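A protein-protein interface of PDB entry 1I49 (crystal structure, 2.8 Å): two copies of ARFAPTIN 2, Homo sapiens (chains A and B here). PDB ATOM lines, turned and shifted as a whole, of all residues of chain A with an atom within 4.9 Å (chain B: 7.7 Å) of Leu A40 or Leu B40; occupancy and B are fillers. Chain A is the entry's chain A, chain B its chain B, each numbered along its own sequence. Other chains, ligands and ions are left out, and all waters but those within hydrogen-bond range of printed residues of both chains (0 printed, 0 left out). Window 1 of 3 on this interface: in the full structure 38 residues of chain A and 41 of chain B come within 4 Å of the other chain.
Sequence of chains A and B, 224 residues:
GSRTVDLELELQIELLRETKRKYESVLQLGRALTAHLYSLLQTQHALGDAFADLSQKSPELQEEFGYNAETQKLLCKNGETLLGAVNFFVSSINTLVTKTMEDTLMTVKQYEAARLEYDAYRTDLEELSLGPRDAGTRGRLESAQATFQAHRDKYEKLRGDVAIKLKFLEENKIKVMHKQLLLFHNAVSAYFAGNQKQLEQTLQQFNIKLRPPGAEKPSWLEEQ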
ATOM      1  N   LEU A  33      -6.792   8.212 -12.467  1.00  0.00           N
ATOM      2  CA  LEU A  33      -6.470   9.472 -13.107  1.00  0.00           C
ATOM      3  C   LEU A  33      -5.951   9.196 -14.521  1.00  0.00           C
ATOM      4  O   LEU A  33      -6.231   9.938 -15.463  1.00  0.00           O
ATOM      5  CB  LEU A  33      -5.412  10.206 -12.295  1.00  0.00           C
ATOM      6  CG  LEU A  33      -4.797  11.415 -12.988  1.00  0.00           C
ATOM      7  CD1 LEU A  33      -5.862  12.471 -13.223  1.00  0.00           C
ATOM      8  CD2 LEU A  33      -3.668  11.957 -12.122  1.00  0.00           C
ATOM      9  N   HIS A  36      -8.924   8.140 -16.842  1.00  0.00           N
ATOM     10  CA  HIS A  36      -9.756   9.289 -17.125  1.00  0.00           C
ATOM     11  C   HIS A  36      -9.124  10.291 -18.085  1.00  0.00           C
ATOM     12  O   HIS A  36      -9.816  10.817 -18.961  1.00  0.00           O
ATOM     13  CB  HIS A  36     -10.157   9.927 -15.805  1.00  0.00           C
ATOM     14  CG  HIS A  36     -10.970   9.009 -14.945  1.00  0.00           C
ATOM     15  ND1 HIS A  36     -11.165   9.215 -13.594  1.00  0.00           N
ATOM     16  CD2 HIS A  36     -11.654   7.879 -15.257  1.00  0.00           C
ATOM     17  CE1 HIS A  36     -11.935   8.250 -13.112  1.00  0.00           C
ATOM     18  NE2 HIS A  36     -12.245   7.427 -14.100  1.00  0.00           N
ATOM     19  N   LEU A  37      -7.824  10.549 -17.949  1.00  0.00           N
ATOM     20  CA  LEU A  37      -7.172  11.481 -18.866  1.00  0.00           C
ATOM     21  C   LEU A  37      -7.238  10.936 -20.274  1.00  0.00           C
ATOM     22  O   LEU A  37      -7.504  11.664 -21.224  1.00  0.00           O
ATOM     23  CB  LEU A  37      -5.705  11.682 -18.520  1.00  0.00           C
ATOM     24  CG  LEU A  37      -5.387  12.595 -17.352  1.00  0.00           C
ATOM     25  CD1 LEU A  37      -3.886  12.743 -17.272  1.00  0.00           C
ATOM     26  CD2 LEU A  37      -6.062  13.945 -17.544  1.00  0.00           C
ATOM     27  N   TYR A  38      -6.980   9.646 -20.401  1.00  0.00           N
ATOM     28  CA  TYR A  38      -7.002   8.999 -21.705  1.00  0.00           C
ATOM     29  C   TYR A  38      -8.392   9.097 -22.316  1.00  0.00           C
ATOM     30  O   TYR A  38      -8.537   9.164 -23.530  1.00  0.00           O
ATOM     31  CB  TYR A  38      -6.599   7.533 -21.570  1.00  0.00           C
ATOM     32  CG  TYR A  38      -6.667   6.750 -22.851  1.00  0.00           C
ATOM     33  CD1 TYR A  38      -5.639   6.819 -23.794  1.00  0.00           C
ATOM     34  CD2 TYR A  38      -7.757   5.922 -23.121  1.00  0.00           C
ATOM     35  CE1 TYR A  38      -5.696   6.072 -24.981  1.00  0.00           C
ATOM     36  CE2 TYR A  38      -7.826   5.176 -24.294  1.00  0.00           C
ATOM     37  CZ  TYR A  38      -6.793   5.252 -25.222  1.00  0.00           C
ATOM     38  OH  TYR A  38      -6.863   4.495 -26.375  1.00  0.00           O
ATOM     39  N   SER A  39      -9.411   9.101 -21.466  1.00  0.00           N
ATOM     40  CA  SER A  39     -10.779   9.199 -21.939  1.00  0.00           C
ATOM     41  C   SER A  39     -11.085  10.623 -22.353  1.00  0.00           C
ATOM     42  O   SER A  39     -11.755  10.869 -23.355  1.00  0.00           O
ATOM     43  CB  SER A  39     -11.753   8.765 -20.846  1.00  0.00           C
ATOM     44  OG  SER A  39     -11.978   7.366 -20.907  1.00  0.00           O
ATOM     45  N   LEU A  40     -10.593  11.565 -21.566  1.00  0.00           N
ATOM     46  CA  LEU A  40     -10.804  12.964 -21.854  1.00  0.00           C
ATOM     47  C   LEU A  40     -10.043  13.308 -23.136  1.00  0.00           C
ATOM     48  O   LEU A  40     -10.491  14.111 -23.943  1.00  0.00           O
ATOM     49  CB  LEU A  40     -10.291  13.797 -20.688  1.00  0.00           C
ATOM     50  CG  LEU A  40     -10.560  15.291 -20.787  1.00  0.00           C
ATOM     51  CD1 LEU A  40     -12.054  15.512 -20.828  1.00  0.00           C
ATOM     52  CD2 LEU A  40      -9.940  16.011 -19.596  1.00  0.00           C
ATOM     53  N   LEU A  41      -8.891  12.682 -23.327  1.00  0.00           N
ATOM     54  CA  LEU A  41      -8.094  12.944 -24.512  1.00  0.00           C
ATOM     55  C   LEU A  41      -8.769  12.459 -25.780  1.00  0.00           C
ATOM     56  O   LEU A  41      -8.769  13.146 -26.789  1.00  0.00           O
ATOM     57  CB  LEU A  41      -6.720  12.275 -24.399  1.00  0.00           C
ATOM     58  CG  LEU A  41      -5.505  13.141 -24.051  1.00  0.00           C
ATOM     59  CD1 LEU A  41      -5.651  13.719 -22.645  1.00  0.00           C
ATOM     60  CD2 LEU A  41      -4.250  12.297 -24.147  1.00  0.00           C
ATOM     61  N   GLN A  42      -9.340  11.266 -25.737  1.00  0.00           N
ATOM     62  CA  GLN A  42      -9.981  10.720 -26.922  1.00  0.00           C
ATOM     63  C   GLN A  42     -11.242  11.488 -27.273  1.00  0.00           C
ATOM     64  O   GLN A  42     -11.601  11.618 -28.444  1.00  0.00           O
ATOM     65  CB  GLN A  42     -10.286   9.235 -26.715  1.00  0.00           C
ATOM     66  CG  GLN A  42      -9.026   8.391 -26.563  1.00  0.00           C
ATOM     67  CD  GLN A  42      -9.075   7.124 -27.391  1.00  0.00           C
ATOM     68  OE1 GLN A  42      -9.867   6.224 -27.119  1.00  0.00           O
ATOM     69  NE2 GLN A  42      -8.231   7.052 -28.417  1.00  0.00           N
ATOM     70  N   THR A  43     -11.903  12.004 -26.243  1.00  0.00           N
ATOM     71  CA  THR A  43     -13.124  12.770 -26.407  1.00  0.00           C
ATOM     72  C   THR A  43     -12.812  14.168 -26.926  1.00  0.00           C
ATOM     73  O   THR A  43     -13.625  14.768 -27.633  1.00  0.00           O
ATOM     74  CB  THR A  43     -13.900  12.846 -25.064  1.00  0.00           C
ATOM     75  OG1 THR A  43     -14.567  11.594 -24.837  1.00  0.00           O
ATOM     76  CG2 THR A  43     -14.925  13.982 -25.074  1.00  0.00           C
ATOM     77  N   GLN A  44     -11.637  14.687 -26.584  1.00  0.00           N
ATOM     78  CA  GLN A  44     -11.259  16.009 -27.061  1.00  0.00           C
ATOM     79  C   GLN A  44     -10.752  15.914 -28.497  1.00  0.00           C
ATOM     80  O   GLN A  44     -10.776  16.893 -29.227  1.00  0.00           O
ATOM     81  CB  GLN A  44     -10.211  16.639 -26.150  1.00  0.00           C
ATOM     82  CG  GLN A  44     -10.722  16.880 -24.735  1.00  0.00           C
ATOM     83  CD  GLN A  44      -9.759  17.688 -23.897  1.00  0.00           C
ATOM     84  OE1 GLN A  44      -8.548  17.481 -23.958  1.00  0.00           O
ATOM     85  NE2 GLN A  44     -10.292  18.610 -23.101  1.00  0.00           N
ATOM     86  N   ALA B  32     -20.052  13.197 -22.967  1.00  0.00           N
ATOM     87  CA  ALA B  32     -18.903  12.382 -22.646  1.00  0.00           C
ATOM     88  C   ALA B  32     -17.912  13.249 -21.878  1.00  0.00           C
ATOM     89  O   ALA B  32     -17.507  12.920 -20.759  1.00  0.00           O
ATOM     90  CB  ALA B  32     -18.272  11.872 -23.918  1.00  0.00           C
ATOM     91  N   LEU B  33     -17.517  14.359 -22.492  1.00  0.00           N
ATOM     92  CA  LEU B  33     -16.583  15.283 -21.865  1.00  0.00           C
ATOM     93  C   LEU B  33     -17.021  15.541 -20.423  1.00  0.00           C
ATOM     94  O   LEU B  33     -16.228  15.485 -19.487  1.00  0.00           O
ATOM     95  CB  LEU B  33     -16.568  16.598 -22.640  1.00  0.00           C
ATOM     96  CG  LEU B  33     -15.706  17.714 -22.056  1.00  0.00           C
ATOM     97  CD1 LEU B  33     -14.256  17.297 -22.089  1.00  0.00           C
ATOM     98  CD2 LEU B  33     -15.910  18.991 -22.848  1.00  0.00           C
ATOM     99  N   THR B  34     -18.302  15.810 -20.254  1.00  0.00           N
ATOM    100  CA  THR B  34     -18.853  16.087 -18.944  1.00  0.00           C
ATOM    101  C   THR B  34     -18.603  14.959 -17.956  1.00  0.00           C
ATOM    102  O   THR B  34     -18.162  15.179 -16.820  1.00  0.00           O
ATOM    103  CB  THR B  34     -20.343  16.330 -19.070  1.00  0.00           C
ATOM    104  OG1 THR B  34     -20.551  17.688 -19.463  1.00  0.00           O
ATOM    105  CG2 THR B  34     -21.046  16.061 -17.770  1.00  0.00           C
ATOM    106  N   ALA B  35     -18.905  13.747 -18.403  1.00  0.00           N
ATOM    107  CA  ALA B  35     -18.737  12.546 -17.604  1.00  0.00           C
ATOM    108  C   ALA B  35     -17.288  12.377 -17.138  1.00  0.00           C
ATOM    109  O   ALA B  35     -17.029  12.192 -15.952  1.00  0.00           O
ATOM    110  CB  ALA B  35     -19.173  11.335 -18.422  1.00  0.00           C
ATOM    111  N   HIS B  36     -16.351  12.446 -18.076  1.00  0.00           N
ATOM    112  CA  HIS B  36     -14.941  12.287 -17.757  1.00  0.00           C
ATOM    113  C   HIS B  36     -14.450  13.371 -16.838  1.00  0.00           C
ATOM    114  O   HIS B  36     -13.600  13.126 -15.986  1.00  0.00           O
ATOM    115  CB  HIS B  36     -14.115  12.286 -19.037  1.00  0.00           C
ATOM    116  CG  HIS B  36     -14.477  11.177 -19.969  1.00  0.00           C
ATOM    117  ND1 HIS B  36     -14.470  11.321 -21.340  1.00  0.00           N
ATOM    118  CD2 HIS B  36     -14.904   9.914 -19.723  1.00  0.00           C
ATOM    119  CE1 HIS B  36     -14.883  10.195 -21.897  1.00  0.00           C
ATOM    120  NE2 HIS B  36     -15.152   9.327 -20.938  1.00  0.00           N
ATOM    121  N   LEU B  37     -14.980  14.574 -17.010  1.00  0.00           N
ATOM    122  CA  LEU B  37     -14.567  15.683 -16.169  1.00  0.00           C
ATOM    123  C   LEU B  37     -15.019  15.440 -14.748  1.00  0.00           C
ATOM    124  O   LEU B  37     -14.305  15.743 -13.793  1.00  0.00           O
ATOM    125  CB  LEU B  37     -15.149  16.997 -16.683  1.00  0.00           C
ATOM    126  CG  LEU B  37     -14.152  17.920 -17.376  1.00  0.00           C
ATOM    127  CD1 LEU B  37     -14.834  19.231 -17.701  1.00  0.00           C
ATOM    128  CD2 LEU B  37     -12.959  18.161 -16.463  1.00  0.00           C
ATOM    129  N   TYR B  38     -16.219  14.899 -14.608  1.00  0.00           N
ATOM    130  CA  TYR B  38     -16.743  14.597 -13.289  1.00  0.00           C
ATOM    131  C   TYR B  38     -15.821  13.543 -12.669  1.00  0.00           C
ATOM    132  O   TYR B  38     -15.445  13.635 -11.504  1.00  0.00           O
ATOM    133  CB  TYR B  38     -18.166  14.046 -13.403  1.00  0.00           C
ATOM    134  CG  TYR B  38     -18.802  13.719 -12.079  1.00  0.00           C
ATOM    135  CD1 TYR B  38     -19.661  14.614 -11.458  1.00  0.00           C
ATOM    136  CD2 TYR B  38     -18.517  12.519 -11.425  1.00  0.00           C
ATOM    137  CE1 TYR B  38     -20.223  14.330 -10.215  1.00  0.00           C
ATOM    138  CE2 TYR B  38     -19.070  12.225 -10.182  1.00  0.00           C
ATOM    139  CZ  TYR B  38     -19.923  13.136  -9.582  1.00  0.00           C
ATOM    140  OH  TYR B  38     -20.466  12.862  -8.347  1.00  0.00           O
ATOM    141  N   SER B  39     -15.459  12.540 -13.460  1.00  0.00           N
ATOM    142  CA  SER B  39     -14.591  11.464 -12.999  1.00  0.00           C
ATOM    143  C   SER B  39     -13.237  11.986 -12.566  1.00  0.00           C
ATOM    144  O   SER B  39     -12.746  11.655 -11.484  1.00  0.00           O
ATOM    145  CB  SER B  39     -14.403  10.424 -14.104  1.00  0.00           C
ATOM    146  OG  SER B  39     -15.513   9.550 -14.151  1.00  0.00           O
ATOM    147  N   LEU B  40     -12.638  12.798 -13.425  1.00  0.00           N
ATOM    148  CA  LEU B  40     -11.336  13.391 -13.165  1.00  0.00           C
ATOM    149  C   LEU B  40     -11.359  14.139 -11.831  1.00  0.00           C
ATOM    150  O   LEU B  40     -10.548  13.874 -10.940  1.00  0.00           O
ATOM    151  CB  LEU B  40     -10.988  14.350 -14.301  1.00  0.00           C
ATOM    152  CG  LEU B  40      -9.519  14.568 -14.637  1.00  0.00           C
ATOM    153  CD1 LEU B  40      -8.818  13.225 -14.801  1.00  0.00           C
ATOM    154  CD2 LEU B  40      -9.428  15.373 -15.924  1.00  0.00           C
ATOM    155  N   LEU B  41     -12.302  15.062 -11.697  1.00  0.00           N
ATOM    156  CA  LEU B  41     -12.434  15.845 -10.477  1.00  0.00           C
ATOM    157  C   LEU B  41     -12.597  14.967  -9.254  1.00  0.00           C
ATOM    158  O   LEU B  41     -12.060  15.264  -8.189  1.00  0.00           O
ATOM    159  CB  LEU B  41     -13.633  16.796 -10.571  1.00  0.00           C
ATOM    160  CG  LEU B  41     -13.340  18.292 -10.711  1.00  0.00           C
ATOM    161  CD1 LEU B  41     -12.564  18.583 -12.007  1.00  0.00           C
ATOM    162  CD2 LEU B  41     -14.655  19.036 -10.697  1.00  0.00           C
ATOM    163  N   GLN B  42     -13.350  13.888  -9.396  1.00  0.00           N
ATOM    164  CA  GLN B  42     -13.567  12.993  -8.272  1.00  0.00           C
ATOM    165  C   GLN B  42     -12.236  12.351  -7.887  1.00  0.00           C
ATOM    166  O   GLN B  42     -11.954  12.129  -6.705  1.00  0.00           O
ATOM    167  CB  GLN B  42     -14.591  11.926  -8.653  1.00  0.00           C
ATOM    168  CG  GLN B  42     -15.031  11.044  -7.505  1.00  0.00           C
ATOM    169  CD  GLN B  42     -16.167  10.118  -7.898  1.00  0.00           C
ATOM    170  OE1 GLN B  42     -17.235  10.574  -8.311  1.00  0.00           O
ATOM    171  NE2 GLN B  42     -15.944   8.813  -7.772  1.00  0.00           N
ATOM    172  N   THR B  43     -11.414  12.085  -8.897  1.00  0.00           N
ATOM    173  CA  THR B  43     -10.114  11.467  -8.700  1.00  0.00           C
ATOM    174  C   THR B  43      -9.046  12.431  -8.210  1.00  0.00           C
ATOM    175  O   THR B  43      -8.092  12.021  -7.550  1.00  0.00           O
ATOM    176  CB  THR B  43      -9.649  10.820  -9.995  1.00  0.00           C
ATOM    177  OG1 THR B  43     -10.574   9.787 -10.336  1.00  0.00           O
ATOM    178  CG2 THR B  43      -8.257  10.226  -9.851  1.00  0.00           C
ATOM    179  N   GLN B  44      -9.197  13.711  -8.536  1.00  0.00           N
ATOM    180  CA  GLN B  44      -8.227  14.704  -8.094  1.00  0.00           C
ATOM    181  C   GLN B  44      -8.504  15.099  -6.657  1.00  0.00           C
ATOM    182  O   GLN B  44      -7.584  15.412  -5.918  1.00  0.00           O
ATOM    183  CB  GLN B  44      -8.249  15.937  -9.000  1.00  0.00           C
ATOM    184  CG  GLN B  44      -7.813  15.627 -10.428  1.00  0.00           C
ATOM    185  CD  GLN B  44      -7.817  16.844 -11.329  1.00  0.00           C
ATOM    186  OE1 GLN B  44      -8.777  17.622 -11.340  1.00  0.00           O
ATOM    187  NE2 GLN B  44      -6.745  17.008 -12.106  1.00  0.00           N
ATOM    188  N   HIS B  45      -9.764  15.074  -6.249  1.00  0.00           N
ATOM    189  CA  HIS B  45     -10.087  15.418  -4.872  1.00  0.00           C
ATOM    190  C   HIS B  45      -9.536  14.348  -3.941  1.00  0.00           C
ATOM    191  O   HIS B  45      -9.047  14.637  -2.851  1.00  0.00           O
ATOM    192  CB  HIS B  45     -11.599  15.519  -4.669  1.00  0.00           C
ATOM    193  CG  HIS B  45     -12.166  16.866  -4.997  1.00  0.00           C
ATOM    194  ND1 HIS B  45     -11.571  18.044  -4.593  1.00  0.00           N
ATOM    195  CD2 HIS B  45     -13.297  17.222  -5.653  1.00  0.00           C
ATOM    196  CE1 HIS B  45     -12.311  19.065  -4.984  1.00  0.00           C
ATOM    197  NE2 HIS B  45     -13.365  18.594  -5.629  1.00  0.00           N
ATOM    198  N   ALA B  46      -9.621  13.101  -4.375  1.00  0.00           N
ATOM    199  CA  ALA B  46      -9.142  11.997  -3.567  1.00  0.00           C
ATOM    200  C   ALA B  46      -7.621  11.980  -3.570  1.00  0.00           C
ATOM    201  O   ALA B  46      -6.998  11.904  -2.511  1.00  0.00           O
ATOM    202  CB  ALA B  46      -9.698  10.694  -4.105  1.00  0.00           C
ATOM    203  N   LEU B  47      -7.023  12.058  -4.755  1.00  0.00           N
ATOM    204  CA  LEU B  47      -5.569  12.060  -4.863  1.00  0.00           C
ATOM    205  C   LEU B  47      -5.037  13.229  -4.040  1.00  0.00           C
ATOM    206  O   LEU B  47      -3.918  13.192  -3.534  1.00  0.00           O
ATOM    207  CB  LEU B  47      -5.143  12.202  -6.329  1.00  0.00           C
ATOM    208  CG  LEU B  47      -3.647  12.105  -6.681  1.00  0.00           C
ATOM    209  CD1 LEU B  47      -3.049  10.852  -6.061  1.00  0.00           C
ATOM    210  CD2 LEU B  47      -3.459  12.067  -8.206  1.00  0.00           C
ATOM    211  N   GLN B  72      -3.340  19.884  -6.367  1.00  0.00           N
ATOM    212  CA  GLN B  72      -4.491  19.070  -6.709  1.00  0.00           C
ATOM    213  C   GLN B  72      -5.763  19.757  -6.209  1.00  0.00           C
ATOM    214  O   GLN B  72      -6.693  19.974  -6.984  1.00  0.00           O
ATOM    215  CB  GLN B  72      -4.340  17.683  -6.082  1.00  0.00           C
ATOM    216  CG  GLN B  72      -4.804  16.533  -6.962  1.00  0.00           C
ATOM    217  CD  GLN B  72      -4.046  16.443  -8.281  1.00  0.00           C
ATOM    218  OE1 GLN B  72      -2.814  16.465  -8.310  1.00  0.00           O
ATOM    219  NE2 GLN B  72      -4.786  16.325  -9.377  1.00  0.00           N
ATOM    220  N   LEU B  75      -6.586  22.654  -8.648  1.00  0.00           N
ATOM    221  CA  LEU B  75      -7.124  22.182  -9.915  1.00  0.00           C
ATOM    222  C   LEU B  75      -8.541  21.625  -9.788  1.00  0.00           C
ATOM    223  O   LEU B  75      -9.129  21.187 -10.780  1.00  0.00           O
ATOM    224  CB  LEU B  75      -6.212  21.098 -10.489  1.00  0.00           C
ATOM    225  CG  LEU B  75      -5.180  21.575 -11.513  1.00  0.00           C
ATOM    226  CD1 LEU B  75      -4.523  22.854 -11.013  1.00  0.00           C
ATOM    227  CD2 LEU B  75      -4.152  20.483 -11.774  1.00  0.00           C
ATOM    228  N   CYS B  76      -9.084  21.645  -8.573  1.00  0.00           N
ATOM    229  CA  CYS B  76     -10.415  21.125  -8.322  1.00  0.00           C
ATOM    230  C   CYS B  76     -11.474  22.185  -8.104  1.00  0.00           C
ATOM    231  O   CYS B  76     -12.664  21.903  -8.209  1.00  0.00           O
ATOM    232  CB  CYS B  76     -10.386  20.178  -7.126  1.00  0.00           C
ATOM    233  SG  CYS B  76      -9.682  18.556  -7.495  1.00  0.00           S
ATOM    234  N   LEU B  82     -15.252  24.984 -14.283  1.00  0.00           N
ATOM    235  CA  LEU B  82     -15.140  24.671 -15.698  1.00  0.00           C
ATOM    236  C   LEU B  82     -16.240  23.697 -16.077  1.00  0.00           C
ATOM    237  O   LEU B  82     -16.783  23.748 -17.178  1.00  0.00           O
ATOM    238  CB  LEU B  82     -13.813  24.013 -16.010  1.00  0.00           C
ATOM    239  CG  LEU B  82     -13.773  23.401 -17.418  1.00  0.00           C
ATOM    240  CD1 LEU B  82     -14.069  24.479 -18.449  1.00  0.00           C
ATOM    241  CD2 LEU B  82     -12.410  22.773 -17.690  1.00  0.00           C
ATOM    242  N   TYR B 191     -10.149  28.499 -17.526  1.00  0.00           N
ATOM    243  CA  TYR B 191      -9.675  27.442 -16.641  1.00  0.00           C
ATOM    244  C   TYR B 191      -8.156  27.575 -16.573  1.00  0.00           C
ATOM    245  O   TYR B 191      -7.595  27.772 -15.499  1.00  0.00           O
ATOM    246  CB  TYR B 191     -10.074  26.080 -17.219  1.00  0.00           C
ATOM    247  CG  TYR B 191      -9.528  24.851 -16.513  1.00  0.00           C
ATOM    248  CD1 TYR B 191      -9.988  24.479 -15.248  1.00  0.00           C
ATOM    249  CD2 TYR B 191      -8.599  24.018 -17.151  1.00  0.00           C
ATOM    250  CE1 TYR B 191      -9.543  23.302 -14.633  1.00  0.00           C
ATOM    251  CE2 TYR B 191      -8.149  22.840 -16.549  1.00  0.00           C
ATOM    252  CZ  TYR B 191      -8.625  22.487 -15.291  1.00  0.00           C
ATOM    253  OH  TYR B 191      -8.183  21.322 -14.699  1.00  0.00           O
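Leu A33 touches Thr B43, and with the chains exchanged Thr A43 touches Leu B33. His A36 touches Ser B39, and with the chains exchanged Ser A39 touches His B36. His A36 touches Thr B43, and with the chains exchanged Thr A43 touches His B36. Leu B40 touches its own counterpart, Leu A40. Of the 14 pairs that touch across the chains among the printed residues, 11 have their exchanged pair printed and touching as well.
OG1 of Thr B43 sits at hydrogen-bond distance from ND1 of His A36 (3.4 Å). A ring nitrogen (ND1) of His B36 lies within hydrogen-bond range of the backbone carbonyl oxygen of Ser A39 (3.4 Å).
O of Ser A39 sits at hydrogen-bond distance from OG1 of Thr A43, 3.3 Å away. O of Ala B32 is in hydrogen-bond range of ND1 of His B36, 3.5 Å away. The backbone carbonyl oxygen (O) of Ser B39 sits at hydrogen-bond distance from the side-chain hydroxyl (OG1) of Thr B43 (3.1 Å).
Of chain B, only Leu B33, His B36 and Leu B40 come within 4 Å of Leu A40. Printed residues of chain B within 4 Å of Thr A43: Ala B32, Leu B33 and His B36. Printed residues of chain A within 4 Å of Thr B43: Leu A33 (3.6 Å) and His A36 (3.4 Å). Of the printed residues of chain A, Leu B33 touches Leu A40 and Thr A43. Printed residues of chain B within 4 Å of Leu A37: Leu B40. Leu B75 touches none of the printed residues of chain A.
Of the 10 printed residues of chain A, 6 touch a printed residue of chain B. Of the 21 printed residues of chain B, 7 touch a printed residue of chain A. Hydrophobic or aromatic side chains of chain B that line the printed part of chain A: Ala B32, Leu B33, His B36, Leu B40 and Leu B47. Among the printed residues, no Asp or Glu carboxylate lies within 4 Å of a Lys or Arg side-chain nitrogen of the other chain.
Leu A33 touches Leu B40. CG2 of Thr B43 touches N of Leu A33, 3.6 Å away. Leu A33 touches Leu B47. CB of His A36 touches CD1 of Leu B40, 3.7 Å away. CD2 of Leu A37 touches CD1 of Leu B40, at 3.95 Å. Leu A40 touches Leu B33. Leu A40 touches Leu B40 (CD2 to CD2, 3.8 Å). Ala B32 touches Thr A43. Thr A43 touches Leu B33. CE1 of His B36 touches OG1 of Thr A43 (3.3 Å).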
